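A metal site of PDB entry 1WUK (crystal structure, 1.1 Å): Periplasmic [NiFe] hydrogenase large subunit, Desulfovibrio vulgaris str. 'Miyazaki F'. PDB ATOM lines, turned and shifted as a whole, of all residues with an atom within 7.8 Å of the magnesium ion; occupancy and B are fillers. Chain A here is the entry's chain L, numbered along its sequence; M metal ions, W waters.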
ATOM      1  N   GLU A  44     -30.797 -21.389 -22.887  1.00  0.00           N
ATOM      2  CA  GLU A  44     -30.312 -20.747 -24.133  1.00  0.00           C
ATOM      3  C   GLU A  44     -29.547 -21.754 -24.986  1.00  0.00           C
ATOM      4  O   GLU A  44     -29.612 -21.687 -26.210  1.00  0.00           O
ATOM      5  CB  GLU A  44     -29.454 -19.524 -23.800  1.00  0.00           C
ATOM      6  CG  GLU A  44     -30.184 -18.384 -23.117  1.00  0.00           C
ATOM      7  CD  GLU A  44     -29.341 -17.518 -22.217  1.00  0.00           C
ATOM      8  OE1 GLU A  44     -28.276 -18.027 -21.721  1.00  0.00           O
ATOM      9  OE2 GLU A  44     -29.755 -16.376 -21.925  1.00  0.00           O
ATOM     10  N   GLU A 319     -23.764  -8.131 -20.917  1.00  0.00           N
ATOM     11  CA  GLU A 319     -23.766  -9.092 -19.829  1.00  0.00           C
ATOM     12  C   GLU A 319     -22.348  -9.618 -19.593  1.00  0.00           C
ATOM     13  O   GLU A 319     -21.734 -10.201 -20.478  1.00  0.00           O
ATOM     14  CB  GLU A 319     -24.706 -10.245 -20.062  1.00  0.00           C
ATOM     15  CG  GLU A 319     -26.153  -9.832 -20.166  1.00  0.00           C
ATOM     16  CD  GLU A 319     -27.015 -11.072 -20.255  1.00  0.00           C
ATOM     17  OE1 GLU A 319     -27.635 -11.456 -19.224  1.00  0.00           O
ATOM     18  OE2 GLU A 319     -27.032 -11.678 -21.367  1.00  0.00           O
ATOM     19  N   TYR A 326     -18.739 -18.907 -16.336  1.00  0.00           N
ATOM     20  CA  TYR A 326     -18.738 -19.026 -17.774  1.00  0.00           C
ATOM     21  C   TYR A 326     -17.325 -18.811 -18.257  1.00  0.00           C
ATOM     22  O   TYR A 326     -16.464 -18.285 -17.560  1.00  0.00           O
ATOM     23  CB  TYR A 326     -19.728 -18.061 -18.488  1.00  0.00           C
ATOM     24  CG  TYR A 326     -21.126 -18.287 -18.014  1.00  0.00           C
ATOM     25  CD1 TYR A 326     -21.674 -17.492 -16.977  1.00  0.00           C
ATOM     26  CD2 TYR A 326     -21.902 -19.298 -18.556  1.00  0.00           C
ATOM     27  CE1 TYR A 326     -22.969 -17.730 -16.544  1.00  0.00           C
ATOM     28  CE2 TYR A 326     -23.195 -19.540 -18.069  1.00  0.00           C
ATOM     29  CZ  TYR A 326     -23.719 -18.753 -17.075  1.00  0.00           C
ATOM     30  OH  TYR A 326     -24.997 -19.039 -16.625  1.00  0.00           O
ATOM     31  N   PRO A 334     -26.642  -8.902 -25.853  1.00  0.00           N
ATOM     32  CA  PRO A 334     -27.343 -10.171 -26.051  1.00  0.00           C
ATOM     33  C   PRO A 334     -27.569 -10.636 -27.455  1.00  0.00           C
ATOM     34  O   PRO A 334     -27.706 -11.840 -27.678  1.00  0.00           O
ATOM     35  CB  PRO A 334     -28.690  -9.973 -25.312  1.00  0.00           C
ATOM     36  CG  PRO A 334     -28.665  -8.632 -24.799  1.00  0.00           C
ATOM     37  CD  PRO A 334     -27.381  -7.986 -25.007  1.00  0.00           C
ATOM     38  N   GLN A 338     -23.295 -15.182 -25.403  1.00  0.00           N
ATOM     39  CA  GLN A 338     -22.629 -16.465 -25.308  1.00  0.00           C
ATOM     40  C   GLN A 338     -22.974 -17.093 -23.982  1.00  0.00           C
ATOM     41  O   GLN A 338     -22.990 -16.390 -22.951  1.00  0.00           O
ATOM     42  CB  GLN A 338     -21.110 -16.307 -25.339  1.00  0.00           C
ATOM     43  CG  GLN A 338     -20.598 -15.735 -26.616  1.00  0.00           C
ATOM     44  CD  GLN A 338     -19.060 -15.641 -26.627  1.00  0.00           C
ATOM     45  OE1 GLN A 338     -18.412 -16.225 -27.521  1.00  0.00           O
ATOM     46  NE2 GLN A 338     -18.555 -14.895 -25.691  1.00  0.00           N
ATOM     47  N   THR A 339     -23.254 -18.396 -24.006  1.00  0.00           N
ATOM     48  CA  THR A 339     -23.585 -19.108 -22.761  1.00  0.00           C
ATOM     49  C   THR A 339     -22.744 -20.385 -22.748  1.00  0.00           C
ATOM     50  O   THR A 339     -23.142 -21.439 -23.270  1.00  0.00           O
ATOM     51  CB  THR A 339     -25.095 -19.405 -22.665  1.00  0.00           C
ATOM     52  OG1 THR A 339     -25.734 -18.150 -22.839  1.00  0.00           O
ATOM     53  CG2 THR A 339     -25.443 -19.995 -21.319  1.00  0.00           C
ATOM     54  N   TRP A 354     -23.831 -18.574 -11.071  1.00  0.00           N
ATOM     55  CA  TRP A 354     -24.309 -18.929 -12.409  1.00  0.00           C
ATOM     56  C   TRP A 354     -25.025 -17.787 -13.105  1.00  0.00           C
ATOM     57  O   TRP A 354     -25.347 -17.911 -14.301  1.00  0.00           O
ATOM     58  CB  TRP A 354     -25.236 -20.168 -12.357  1.00  0.00           C
ATOM     59  CG  TRP A 354     -24.486 -21.445 -12.082  1.00  0.00           C
ATOM     60  CD1 TRP A 354     -24.553 -22.205 -10.956  1.00  0.00           C
ATOM     61  CD2 TRP A 354     -23.589 -22.100 -12.978  1.00  0.00           C
ATOM     62  NE1 TRP A 354     -23.751 -23.306 -11.084  1.00  0.00           N
ATOM     63  CE2 TRP A 354     -23.144 -23.261 -12.323  1.00  0.00           C
ATOM     64  CE3 TRP A 354     -23.126 -21.822 -14.281  1.00  0.00           C
ATOM     65  CZ2 TRP A 354     -22.242 -24.151 -12.927  1.00  0.00           C
ATOM     66  CZ3 TRP A 354     -22.233 -22.682 -14.868  1.00  0.00           C
ATOM     67  CH2 TRP A 354     -21.805 -23.803 -14.200  1.00  0.00           C
ATOM     68  N   LYS A 356     -25.059 -14.307 -15.066  1.00  0.00           N
ATOM     69  CA  LYS A 356     -24.295 -13.229 -15.681  1.00  0.00           C
ATOM     70  C   LYS A 356     -24.572 -11.921 -14.944  1.00  0.00           C
ATOM     71  O   LYS A 356     -25.474 -11.839 -14.102  1.00  0.00           O
ATOM     72  CB  LYS A 356     -24.629 -13.126 -17.170  1.00  0.00           C
ATOM     73  CG  LYS A 356     -24.385 -14.403 -17.998  1.00  0.00           C
ATOM     74  CD  LYS A 356     -24.810 -14.221 -19.438  1.00  0.00           C
ATOM     75  CE  LYS A 356     -24.586 -15.486 -20.244  1.00  0.00           C
ATOM     76  NZ  LYS A 356     -25.247 -15.391 -21.561  1.00  0.00           N
ATOM     77  N   PRO A 358     -25.466  -8.230 -15.846  1.00  0.00           N
ATOM     78  CA  PRO A 358     -25.854  -7.233 -16.851  1.00  0.00           C
ATOM     79  C   PRO A 358     -25.466  -5.851 -16.329  1.00  0.00           C
ATOM     80  O   PRO A 358     -25.669  -5.520 -15.161  1.00  0.00           O
ATOM     81  CB  PRO A 358     -27.353  -7.390 -16.973  1.00  0.00           C
ATOM     82  CG  PRO A 358     -27.689  -8.688 -16.316  1.00  0.00           C
ATOM     83  CD  PRO A 358     -26.662  -8.819 -15.238  1.00  0.00           C
ATOM     84  N   SER A 465     -36.016  -8.977 -21.108  1.00  0.00           N
ATOM     85  CA  SER A 465     -35.834  -8.910 -22.560  1.00  0.00           C
ATOM     86  C   SER A 465     -35.375 -10.276 -23.058  1.00  0.00           C
ATOM     87  O   SER A 465     -34.515 -10.952 -22.452  1.00  0.00           O
ATOM     88  CB  SER A 465     -34.892  -7.762 -22.937  1.00  0.00           C
ATOM     89  OG  SER A 465     -33.626  -7.816 -22.309  1.00  0.00           O
ATOM     90  N   TRP A 467     -34.024 -11.991 -26.759  1.00  0.00           N
ATOM     91  CA  TRP A 467     -33.270 -11.552 -27.953  1.00  0.00           C
ATOM     92  C   TRP A 467     -33.014 -12.756 -28.872  1.00  0.00           C
ATOM     93  O   TRP A 467     -32.391 -13.700 -28.455  1.00  0.00           O
ATOM     94  CB  TRP A 467     -31.951 -10.960 -27.508  1.00  0.00           C
ATOM     95  CG  TRP A 467     -32.011  -9.866 -26.495  1.00  0.00           C
ATOM     96  CD1 TRP A 467     -32.232 -10.009 -25.176  1.00  0.00           C
ATOM     97  CD2 TRP A 467     -31.850  -8.481 -26.746  1.00  0.00           C
ATOM     98  NE1 TRP A 467     -32.199  -8.766 -24.554  1.00  0.00           N
ATOM     99  CE2 TRP A 467     -31.963  -7.826 -25.500  1.00  0.00           C
ATOM    100  CE3 TRP A 467     -31.578  -7.715 -27.904  1.00  0.00           C
ATOM    101  CZ2 TRP A 467     -31.832  -6.433 -25.420  1.00  0.00           C
ATOM    102  CZ3 TRP A 467     -31.452  -6.375 -27.816  1.00  0.00           C
ATOM    103  CH2 TRP A 467     -31.578  -5.760 -26.541  1.00  0.00           C
ATOM    104  N   PHE A 478     -30.394 -17.340 -29.048  1.00  0.00           N
ATOM    105  CA  PHE A 478     -31.525 -16.870 -28.253  1.00  0.00           C
ATOM    106  C   PHE A 478     -30.971 -16.556 -26.873  1.00  0.00           C
ATOM    107  O   PHE A 478     -30.388 -17.424 -26.225  1.00  0.00           O
ATOM    108  CB  PHE A 478     -32.652 -17.909 -28.179  1.00  0.00           C
ATOM    109  CG  PHE A 478     -33.999 -17.311 -27.832  1.00  0.00           C
ATOM    110  CD1 PHE A 478     -34.280 -16.895 -26.532  1.00  0.00           C
ATOM    111  CD2 PHE A 478     -34.959 -17.146 -28.816  1.00  0.00           C
ATOM    112  CE1 PHE A 478     -35.513 -16.298 -26.246  1.00  0.00           C
ATOM    113  CE2 PHE A 478     -36.169 -16.557 -28.526  1.00  0.00           C
ATOM    114  CZ  PHE A 478     -36.444 -16.134 -27.225  1.00  0.00           C
ATOM    115  N   GLN A 479     -31.124 -15.312 -26.427  1.00  0.00           N
ATOM    116  CA  GLN A 479     -30.594 -14.878 -25.141  1.00  0.00           C
ATOM    117  C   GLN A 479     -31.685 -14.257 -24.323  1.00  0.00           C
ATOM    118  O   GLN A 479     -32.421 -13.378 -24.783  1.00  0.00           O
ATOM    119  CB  GLN A 479     -29.427 -13.894 -25.333  1.00  0.00           C
ATOM    120  CG  GLN A 479     -28.213 -14.560 -26.006  1.00  0.00           C
ATOM    121  CD  GLN A 479     -27.445 -15.484 -25.141  1.00  0.00           C
ATOM    122  OE1 GLN A 479     -27.318 -15.263 -23.908  1.00  0.00           O
ATOM    123  NE2 GLN A 479     -26.849 -16.512 -25.701  1.00  0.00           N
ATOM    124  N   LEU A 480     -31.766 -14.673 -23.062  1.00  0.00           N
ATOM    125  CA  LEU A 480     -32.663 -14.064 -22.064  1.00  0.00           C
ATOM    126  C   LEU A 480     -31.817 -13.181 -21.180  1.00  0.00           C
ATOM    127  O   LEU A 480     -30.779 -13.620 -20.653  1.00  0.00           O
ATOM    128  CB  LEU A 480     -33.368 -15.103 -21.213  1.00  0.00           C
ATOM    129  CG  LEU A 480     -34.252 -16.101 -21.884  1.00  0.00           C
ATOM    130  CD1 LEU A 480     -33.638 -17.142 -22.720  1.00  0.00           C
ATOM    131  CD2 LEU A 480     -35.119 -16.806 -20.791  1.00  0.00           C
ATOM    132  N   VAL A 481     -32.272 -11.971 -20.901  1.00  0.00           N
ATOM    133  CA  VAL A 481     -31.672 -11.067 -19.904  1.00  0.00           C
ATOM    134  C   VAL A 481     -32.830 -10.700 -18.962  1.00  0.00           C
ATOM    135  O   VAL A 481     -33.800 -10.079 -19.387  1.00  0.00           O
ATOM    136  CB  VAL A 481     -31.063  -9.807 -20.517  1.00  0.00           C
ATOM    137  CG1 VAL A 481     -30.326  -9.012 -19.435  1.00  0.00           C
ATOM    138  CG2 VAL A 481     -30.173 -10.150 -21.686  1.00  0.00           C
ATOM    139  N   VAL A 482     -32.765 -11.194 -17.705  1.00  0.00           N
ATOM    140  CA  VAL A 482     -33.976 -11.306 -16.893  1.00  0.00           C
ATOM    141  C   VAL A 482     -33.861 -10.352 -15.716  1.00  0.00           C
ATOM    142  O   VAL A 482     -32.755  -9.982 -15.315  1.00  0.00           O
ATOM    143  CB  VAL A 482     -34.157 -12.792 -16.529  1.00  0.00           C
ATOM    144  CG1 VAL A 482     -35.450 -13.082 -15.802  1.00  0.00           C
ATOM    145  CG2 VAL A 482     -34.127 -13.620 -17.777  1.00  0.00           C
ATOM    146  N   THR A 485     -31.514 -11.182 -13.069  1.00  0.00           N
ATOM    147  CA  THR A 485     -30.135 -11.144 -13.509  1.00  0.00           C
ATOM    148  C   THR A 485     -29.544  -9.763 -13.218  1.00  0.00           C
ATOM    149  O   THR A 485     -28.410  -9.630 -12.716  1.00  0.00           O
ATOM    150  CB  THR A 485     -30.016 -11.480 -15.040  1.00  0.00           C
ATOM    151  OG1 THR A 485     -30.928 -12.496 -15.439  1.00  0.00           O
ATOM    152  CG2 THR A 485     -28.598 -11.919 -15.345  1.00  0.00           C
ATOM    153  N   CYS A 531     -35.220 -17.552 -12.961  1.00  0.00           N
ATOM    154  CA  CYS A 531     -35.223 -16.410 -13.863  1.00  0.00           C
ATOM    155  C   CYS A 531     -33.836 -15.903 -14.097  1.00  0.00           C
ATOM    156  O   CYS A 531     -33.405 -15.687 -15.242  1.00  0.00           O
ATOM    157  CB  CYS A 531     -36.095 -15.260 -13.292  1.00  0.00           C
ATOM    158  SG  CYS A 531     -37.803 -15.369 -13.893  1.00  0.00           S
ATOM    159  N   GLY A 532     -33.092 -15.634 -13.036  1.00  0.00           N
ATOM    160  CA  GLY A 532     -31.837 -14.933 -13.198  1.00  0.00           C
ATOM    161  C   GLY A 532     -30.821 -15.736 -14.013  1.00  0.00           C
ATOM    162  O   GLY A 532     -30.047 -15.134 -14.771  1.00  0.00           O
ATOM    163  N   VAL A 533     -30.817 -17.052 -13.843  1.00  0.00           N
ATOM    164  CA  VAL A 533     -29.844 -17.924 -14.488  1.00  0.00           C
ATOM    165  C   VAL A 533     -30.323 -18.593 -15.747  1.00  0.00           C
ATOM    166  O   VAL A 533     -29.597 -18.684 -16.760  1.00  0.00           O
ATOM    167  CB  VAL A 533     -29.357 -19.051 -13.527  1.00  0.00           C
ATOM    168  CG1 VAL A 533     -28.364 -19.947 -14.247  1.00  0.00           C
ATOM    169  CG2 VAL A 533     -28.769 -18.507 -12.231  1.00  0.00           C
ATOM    170  N   HIS A 534     -31.550 -19.124 -15.767  1.00  0.00           N
ATOM    171  CA  HIS A 534     -32.106 -19.885 -16.861  1.00  0.00           C
ATOM    172  C   HIS A 534     -31.077 -20.949 -17.365  1.00  0.00           C
ATOM    173  O   HIS A 534     -30.477 -21.651 -16.497  1.00  0.00           O
ATOM    174  CB  HIS A 534     -32.719 -18.977 -17.952  1.00  0.00           C
ATOM    175  CG  HIS A 534     -31.957 -17.735 -18.287  1.00  0.00           C
ATOM    176  ND1 HIS A 534     -32.003 -16.612 -17.491  1.00  0.00           N
ATOM    177  CD2 HIS A 534     -31.046 -17.454 -19.254  1.00  0.00           C
ATOM    178  CE1 HIS A 534     -31.156 -15.709 -17.962  1.00  0.00           C
ATOM    179  NE2 HIS A 534     -30.562 -16.180 -19.061  1.00  0.00           N
ATOM    180  OXT HIS A 534     -30.954 -21.093 -18.591  1.00  0.00           O
HETATM  181 MG    MG M   1     -29.238 -15.050 -20.314  1.00  0.00          MG
HETATM  182  O   HOH W   1     -27.609 -16.308 -19.849  1.00  0.00           O
HETATM  183  O   HOH W   2     -28.679 -13.824 -18.718  1.00  0.00           O
HETATM  184  O   HOH W   3     -28.027 -14.058 -21.636  1.00  0.00           O
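The nearest printed residue that does not touch the magnesium ion is Gln 479 (4.1 Å).
The side-chain carboxylate (OE1) of Glu 44 sits at hydrogen-bond distance from the side-chain hydroxyl (OG1) of Thr 339, at 2.8 Å. A ring nitrogen (ND1) of His 534 sits at hydrogen-bond distance from the backbone carbonyl oxygen (O) of Cys 531 (2.8 Å). The side-chain amide oxygen of Gln 479 sits close to the side-chain carboxylate of Glu 44 (3.3 Å).
The magnesium ion is bound by water W3 (2.0 Å), water W2 (2.1 Å), water W1 (2.1 Å), O of Leu 480 (2.1 Å), NE2 of His 534 (2.1 Å) and OE2 of Glu 44 (2.1 Å).
Water W1 lies within hydrogen-bond range of OE1 of Glu 44 (2.6 Å) and NZ of Lys 356 (3.1 Å). Water W3 lies within hydrogen-bond range of the side-chain carboxylate (OE2) of Glu 319 (2.6 Å), the side-chain amide oxygen (OE1) of Gln 479 (2.7 Å) and the side-chain amino group (NZ) of Lys 356 (3.1 Å).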
